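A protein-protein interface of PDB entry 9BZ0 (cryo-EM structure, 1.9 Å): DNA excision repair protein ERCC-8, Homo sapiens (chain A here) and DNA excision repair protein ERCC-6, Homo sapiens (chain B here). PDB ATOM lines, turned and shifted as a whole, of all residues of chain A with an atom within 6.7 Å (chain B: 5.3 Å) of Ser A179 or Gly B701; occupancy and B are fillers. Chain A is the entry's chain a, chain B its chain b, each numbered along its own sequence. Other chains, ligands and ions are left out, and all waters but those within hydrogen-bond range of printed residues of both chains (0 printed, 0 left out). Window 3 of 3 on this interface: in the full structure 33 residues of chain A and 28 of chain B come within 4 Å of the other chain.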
ATOM      1  N   LYS A 167      14.884   9.923 -18.510  1.00  0.00           N
ATOM      2  CA  LYS A 167      14.654   9.345 -19.826  1.00  0.00           C
ATOM      3  C   LYS A 167      14.068   7.945 -19.715  1.00  0.00           C
ATOM      4  O   LYS A 167      14.624   7.089 -19.024  1.00  0.00           O
ATOM      5  CB  LYS A 167      15.960   9.273 -20.610  1.00  0.00           C
ATOM      6  CG  LYS A 167      16.714  10.561 -20.677  1.00  0.00           C
ATOM      7  CD  LYS A 167      17.890  10.443 -21.608  1.00  0.00           C
ATOM      8  CE  LYS A 167      18.689  11.728 -21.643  1.00  0.00           C
ATOM      9  NZ  LYS A 167      19.766  11.684 -22.672  1.00  0.00           N
ATOM     10  N   GLN A 169      13.473   4.249 -20.910  1.00  0.00           N
ATOM     11  CA  GLN A 169      14.316   3.329 -21.646  1.00  0.00           C
ATOM     12  C   GLN A 169      13.491   2.167 -22.168  1.00  0.00           C
ATOM     13  O   GLN A 169      12.501   1.762 -21.560  1.00  0.00           O
ATOM     14  CB  GLN A 169      15.471   2.828 -20.811  1.00  0.00           C
ATOM     15  CG  GLN A 169      16.265   3.950 -20.209  1.00  0.00           C
ATOM     16  CD  GLN A 169      17.707   3.601 -20.013  1.00  0.00           C
ATOM     17  OE1 GLN A 169      18.228   2.693 -20.653  1.00  0.00           O
ATOM     18  NE2 GLN A 169      18.373   4.325 -19.128  1.00  0.00           N
ATOM     19  N   LEU A 170      13.909   1.641 -23.309  1.00  0.00           N
ATOM     20  CA  LEU A 170      13.243   0.536 -23.974  1.00  0.00           C
ATOM     21  C   LEU A 170      14.248  -0.579 -24.204  1.00  0.00           C
ATOM     22  O   LEU A 170      15.260  -0.371 -24.877  1.00  0.00           O
ATOM     23  CB  LEU A 170      12.660   1.002 -25.299  1.00  0.00           C
ATOM     24  CG  LEU A 170      11.494   1.967 -25.240  1.00  0.00           C
ATOM     25  CD1 LEU A 170      11.275   2.572 -26.588  1.00  0.00           C
ATOM     26  CD2 LEU A 170      10.257   1.284 -24.761  1.00  0.00           C
ATOM     27  N   CYS A 171      13.979  -1.754 -23.655  1.00  0.00           N
ATOM     28  CA  CYS A 171      14.812  -2.928 -23.864  1.00  0.00           C
ATOM     29  C   CYS A 171      14.108  -3.897 -24.796  1.00  0.00           C
ATOM     30  O   CYS A 171      12.965  -4.285 -24.545  1.00  0.00           O
ATOM     31  CB  CYS A 171      15.135  -3.612 -22.542  1.00  0.00           C
ATOM     32  SG  CYS A 171      15.969  -2.565 -21.367  1.00  0.00           S
ATOM     33  N   GLY A 176      18.259  -7.991 -27.641  1.00  0.00           N
ATOM     34  CA  GLY A 176      19.130  -7.660 -26.539  1.00  0.00           C
ATOM     35  C   GLY A 176      19.468  -6.199 -26.441  1.00  0.00           C
ATOM     36  O   GLY A 176      20.214  -5.812 -25.543  1.00  0.00           O
ATOM     37  N   SER A 177      18.931  -5.384 -27.335  1.00  0.00           N
ATOM     38  CA  SER A 177      19.142  -3.945 -27.321  1.00  0.00           C
ATOM     39  C   SER A 177      18.624  -3.305 -26.047  1.00  0.00           C
ATOM     40  O   SER A 177      17.537  -3.629 -25.570  1.00  0.00           O
ATOM     41  CB  SER A 177      18.442  -3.315 -28.512  1.00  0.00           C
ATOM     42  OG  SER A 177      18.561  -1.907 -28.469  1.00  0.00           O
ATOM     43  N   CYS A 178      19.404  -2.385 -25.498  1.00  0.00           N
ATOM     44  CA  CYS A 178      18.904  -1.537 -24.427  1.00  0.00           C
ATOM     45  C   CYS A 178      19.285  -0.075 -24.609  1.00  0.00           C
ATOM     46  O   CYS A 178      19.166   0.701 -23.660  1.00  0.00           O
ATOM     47  CB  CYS A 178      19.410  -2.045 -23.082  1.00  0.00           C
ATOM     48  SG  CYS A 178      21.196  -2.017 -22.898  1.00  0.00           S
ATOM     49  N   SER A 179      19.747   0.317 -25.790  1.00  0.00           N
ATOM     50  CA  SER A 179      20.224   1.667 -26.053  1.00  0.00           C
ATOM     51  C   SER A 179      19.130   2.711 -26.253  1.00  0.00           C
ATOM     52  O   SER A 179      19.392   3.898 -26.051  1.00  0.00           O
ATOM     53  CB  SER A 179      21.143   1.645 -27.272  1.00  0.00           C
ATOM     54  OG  SER A 179      20.456   1.199 -28.421  1.00  0.00           O
ATOM     55  N   HIS A 180      17.921   2.311 -26.629  1.00  0.00           N
ATOM     56  CA  HIS A 180      16.884   3.254 -27.044  1.00  0.00           C
ATOM     57  C   HIS A 180      16.295   4.017 -25.863  1.00  0.00           C
ATOM     58  O   HIS A 180      15.788   3.416 -24.916  1.00  0.00           O
ATOM     59  CB  HIS A 180      15.810   2.490 -27.803  1.00  0.00           C
ATOM     60  CG  HIS A 180      14.781   3.355 -28.446  1.00  0.00           C
ATOM     61  ND1 HIS A 180      13.651   2.843 -29.034  1.00  0.00           N
ATOM     62  CD2 HIS A 180      14.708   4.694 -28.598  1.00  0.00           C
ATOM     63  CE1 HIS A 180      12.929   3.828 -29.527  1.00  0.00           C
ATOM     64  NE2 HIS A 180      13.545   4.962 -29.271  1.00  0.00           N
ATOM     65  N   ILE A 181      16.359   5.345 -25.929  1.00  0.00           N
ATOM     66  CA  ILE A 181      15.863   6.247 -24.901  1.00  0.00           C
ATOM     67  C   ILE A 181      14.832   7.196 -25.490  1.00  0.00           C
ATOM     68  O   ILE A 181      14.898   7.557 -26.666  1.00  0.00           O
ATOM     69  CB  ILE A 181      17.012   7.052 -24.263  1.00  0.00           C
ATOM     70  CG1 ILE A 181      17.671   7.949 -25.308  1.00  0.00           C
ATOM     71  CG2 ILE A 181      18.030   6.137 -23.649  1.00  0.00           C
ATOM     72  CD1 ILE A 181      18.896   8.655 -24.830  1.00  0.00           C
ATOM     73  N   GLN A 183      13.185  11.023 -24.660  1.00  0.00           N
ATOM     74  CA  GLN A 183      13.890  12.147 -24.046  1.00  0.00           C
ATOM     75  C   GLN A 183      12.994  13.317 -23.645  1.00  0.00           C
ATOM     76  O   GLN A 183      13.483  14.443 -23.535  1.00  0.00           O
ATOM     77  CB  GLN A 183      14.996  12.654 -24.970  1.00  0.00           C
ATOM     78  CG  GLN A 183      15.952  11.587 -25.440  1.00  0.00           C
ATOM     79  CD  GLN A 183      17.270  12.161 -25.909  1.00  0.00           C
ATOM     80  OE1 GLN A 183      18.267  12.128 -25.187  1.00  0.00           O
ATOM     81  NE2 GLN A 183      17.286  12.689 -27.127  1.00  0.00           N
ATOM     82  N   TRP B 689      27.594   6.357 -34.705  1.00  0.00           N
ATOM     83  CA  TRP B 689      26.728   7.027 -33.747  1.00  0.00           C
ATOM     84  C   TRP B 689      26.226   8.351 -34.283  1.00  0.00           C
ATOM     85  O   TRP B 689      25.053   8.681 -34.121  1.00  0.00           O
ATOM     86  CB  TRP B 689      27.424   7.251 -32.411  1.00  0.00           C
ATOM     87  CG  TRP B 689      26.486   7.865 -31.418  1.00  0.00           C
ATOM     88  CD1 TRP B 689      25.666   7.201 -30.577  1.00  0.00           C
ATOM     89  CD2 TRP B 689      26.230   9.249 -31.207  1.00  0.00           C
ATOM     90  NE1 TRP B 689      24.930   8.072 -29.844  1.00  0.00           N
ATOM     91  CE2 TRP B 689      25.253   9.342 -30.216  1.00  0.00           C
ATOM     92  CE3 TRP B 689      26.733  10.421 -31.760  1.00  0.00           C
ATOM     93  CZ2 TRP B 689      24.775  10.547 -29.761  1.00  0.00           C
ATOM     94  CZ3 TRP B 689      26.254  11.613 -31.308  1.00  0.00           C
ATOM     95  CH2 TRP B 689      25.288  11.671 -30.319  1.00  0.00           C
ATOM     96  N   ASP B 693      22.389   9.299 -34.834  1.00  0.00           N
ATOM     97  CA  ASP B 693      21.831  10.392 -34.064  1.00  0.00           C
ATOM     98  C   ASP B 693      21.201  11.446 -34.945  1.00  0.00           C
ATOM     99  O   ASP B 693      20.367  12.213 -34.466  1.00  0.00           O
ATOM    100  CB  ASP B 693      22.925  11.002 -33.196  1.00  0.00           C
ATOM    101  CG  ASP B 693      22.436  12.156 -32.364  1.00  0.00           C
ATOM    102  OD1 ASP B 693      21.488  11.970 -31.581  1.00  0.00           O
ATOM    103  OD2 ASP B 693      23.007  13.259 -32.481  1.00  0.00           O
ATOM    104  N   GLY B 698      18.354   9.234 -30.285  1.00  0.00           N
ATOM    105  CA  GLY B 698      18.094   8.420 -29.129  1.00  0.00           C
ATOM    106  C   GLY B 698      18.031   6.938 -29.373  1.00  0.00           C
ATOM    107  O   GLY B 698      17.950   6.180 -28.410  1.00  0.00           O
ATOM    108  N   LYS B 699      18.086   6.491 -30.622  1.00  0.00           N
ATOM    109  CA  LYS B 699      18.077   5.061 -30.890  1.00  0.00           C
ATOM    110  C   LYS B 699      19.315   4.379 -30.327  1.00  0.00           C
ATOM    111  O   LYS B 699      19.218   3.334 -29.678  1.00  0.00           O
ATOM    112  CB  LYS B 699      17.966   4.813 -32.387  1.00  0.00           C
ATOM    113  CG  LYS B 699      17.660   3.391 -32.736  1.00  0.00           C
ATOM    114  CD  LYS B 699      16.201   3.139 -32.548  1.00  0.00           C
ATOM    115  CE  LYS B 699      15.859   1.703 -32.721  1.00  0.00           C
ATOM    116  NZ  LYS B 699      14.392   1.548 -32.764  1.00  0.00           N
ATOM    117  N   LEU B 700      20.490   4.949 -30.561  1.00  0.00           N
ATOM    118  CA  LEU B 700      21.720   4.430 -29.990  1.00  0.00           C
ATOM    119  C   LEU B 700      22.078   5.062 -28.656  1.00  0.00           C
ATOM    120  O   LEU B 700      23.187   4.852 -28.165  1.00  0.00           O
ATOM    121  CB  LEU B 700      22.869   4.590 -30.978  1.00  0.00           C
ATOM    122  CG  LEU B 700      22.723   3.803 -32.271  1.00  0.00           C
ATOM    123  CD1 LEU B 700      23.936   3.957 -33.125  1.00  0.00           C
ATOM    124  CD2 LEU B 700      22.511   2.362 -31.960  1.00  0.00           C
ATOM    125  N   GLY B 701      21.175   5.803 -28.054  1.00  0.00           N
ATOM    126  CA  GLY B 701      21.469   6.495 -26.823  1.00  0.00           C
ATOM    127  C   GLY B 701      22.383   7.689 -27.020  1.00  0.00           C
ATOM    128  O   GLY B 701      22.598   8.176 -28.121  1.00  0.00           O
ATOM    129  N   THR B 702      22.914   8.168 -25.902  1.00  0.00           N
ATOM    130  CA  THR B 702      23.906   9.227 -25.930  1.00  0.00           C
ATOM    131  C   THR B 702      25.281   8.694 -26.299  1.00  0.00           C
ATOM    132  O   THR B 702      25.594   7.518 -26.109  1.00  0.00           O
ATOM    133  CB  THR B 702      23.975   9.930 -24.582  1.00  0.00           C
ATOM    134  OG1 THR B 702      24.426   9.010 -23.587  1.00  0.00           O
ATOM    135  CG2 THR B 702      22.607  10.426 -24.199  1.00  0.00           C
ATOM    136  N   LEU B 703      26.101   9.582 -26.850  1.00  0.00           N
ATOM    137  CA  LEU B 703      27.433   9.187 -27.300  1.00  0.00           C
ATOM    138  C   LEU B 703      28.294   8.583 -26.203  1.00  0.00           C
ATOM    139  O   LEU B 703      28.950   7.563 -26.466  1.00  0.00           O
ATOM    140  CB  LEU B 703      28.116  10.378 -27.970  1.00  0.00           C
ATOM    141  CG  LEU B 703      29.536  10.158 -28.469  1.00  0.00           C
ATOM    142  CD1 LEU B 703      29.564   9.108 -29.540  1.00  0.00           C
ATOM    143  CD2 LEU B 703      30.060  11.454 -29.005  1.00  0.00           C
ATOM    144  N   GLN B 709      29.350   1.157 -24.258  1.00  0.00           N
ATOM    145  CA  GLN B 709      28.644  -0.091 -24.518  1.00  0.00           C
ATOM    146  C   GLN B 709      29.038  -0.803 -25.802  1.00  0.00           C
ATOM    147  O   GLN B 709      28.866  -2.020 -25.881  1.00  0.00           O
ATOM    148  CB  GLN B 709      27.140   0.162 -24.557  1.00  0.00           C
ATOM    149  CG  GLN B 709      26.534   0.506 -23.226  1.00  0.00           C
ATOM    150  CD  GLN B 709      25.027   0.606 -23.288  1.00  0.00           C
ATOM    151  OE1 GLN B 709      24.435   0.566 -24.366  1.00  0.00           O
ATOM    152  NE2 GLN B 709      24.394   0.739 -22.128  1.00  0.00           N
ATOM    153  N   PHE B 710      29.569  -0.106 -26.798  1.00  0.00           N
ATOM    154  CA  PHE B 710      29.831  -0.732 -28.086  1.00  0.00           C
ATOM    155  C   PHE B 710      31.229  -0.467 -28.615  1.00  0.00           C
ATOM    156  O   PHE B 710      31.913  -1.403 -29.029  1.00  0.00           O
ATOM    157  CB  PHE B 710      28.803  -0.298 -29.121  1.00  0.00           C
ATOM    158  CG  PHE B 710      27.415  -0.718 -28.806  1.00  0.00           C
ATOM    159  CD1 PHE B 710      27.037  -2.023 -28.992  1.00  0.00           C
ATOM    160  CD2 PHE B 710      26.486   0.174 -28.344  1.00  0.00           C
ATOM    161  CE1 PHE B 710      25.778  -2.428 -28.719  1.00  0.00           C
ATOM    162  CE2 PHE B 710      25.219  -0.236 -28.067  1.00  0.00           C
ATOM    163  CZ  PHE B 710      24.867  -1.537 -28.252  1.00  0.00           C
ATOM    164  N   THR B 740      20.295  -3.792 -33.820  1.00  0.00           N
ATOM    165  CA  THR B 740      19.672  -2.489 -33.592  1.00  0.00           C
ATOM    166  C   THR B 740      19.633  -1.631 -34.843  1.00  0.00           C
ATOM    167  O   THR B 740      18.629  -0.966 -35.103  1.00  0.00           O
ATOM    168  CB  THR B 740      20.389  -1.722 -32.489  1.00  0.00           C
ATOM    169  OG1 THR B 740      21.764  -1.548 -32.849  1.00  0.00           O
ATOM    170  CG2 THR B 740      20.330  -2.465 -31.218  1.00  0.00           C
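The backbone carbonyl oxygen of Lys B699 lies within hydrogen-bond range of the side-chain hydroxyl of Ser A179 (2.8 Å). O of Ser A179 is in hydrogen-bond range of N of Gly B701, at 3.3 Å. The backbone NH (N) of His A180 lies within hydrogen-bond range of the backbone carbonyl oxygen (O) of Lys B699 (3.5 Å). N of Ile A181 is in hydrogen-bond range of O of Gly B698, at 3.1 Å.
Hydrophobic or aromatic side chains of chain A that line the printed part of chain B: His A180 and Ile A181. Of the 11 printed residues of chain B, 6 touch a printed residue of chain A. Among the printed residues, 10 pairs touch across the chains. Among the printed residues, no Asp or Glu carboxylate lies within 4 Å of a Lys or Arg side-chain nitrogen of the other chain.
Ser A179 touches four residues of chain B. Of chain A, only Ser A179 and Ile A181 come within 4 Å of Gly B701. Of the printed residues of chain B, His A180 touches Gly B698 (3.4 Å) and Lys B699 (3.5 Å). Of the printed residues of chain A, Thr B740 touches Ser A177 (3.3 Å). Printed residues of chain A within 4 Å of Thr B702: Lys A167 (3.5 Å). Gln B709 touches none of the printed residues of chain A. The nearest residue of chain B that does not touch Ser A179 is Gln B709 (4.5 Å). The nearest residue of chain A that does not touch Gly B701 is His A180 (5.0 Å). The nearest printed residue of chain A that does not touch Lys B699 is Ile A181 (5.1 Å).
Among the printed residues, pairs that only touch across the chains: Ser A177 with Thr B740 (3.3 Å), His A180 with Gly B698 (3.4 Å), Lys A167 with Thr B702 (3.5 Å), Ser A179 with Gly B698 (3.6 Å), Ser A179 with Leu B700 (3.8 Å) and Ile A181 with Gly B701 (3.9 Å).
The side-chain amide oxygen of Gln A183 is in hydrogen-bond range of the side-chain amino group of Lys A167 (3.0 Å). N of Leu A170 sits at hydrogen-bond distance from O of His A180 (3.0 Å). NE1 of Trp B689 lies within hydrogen-bond range of O of Gly B701, 2.9 Å away.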
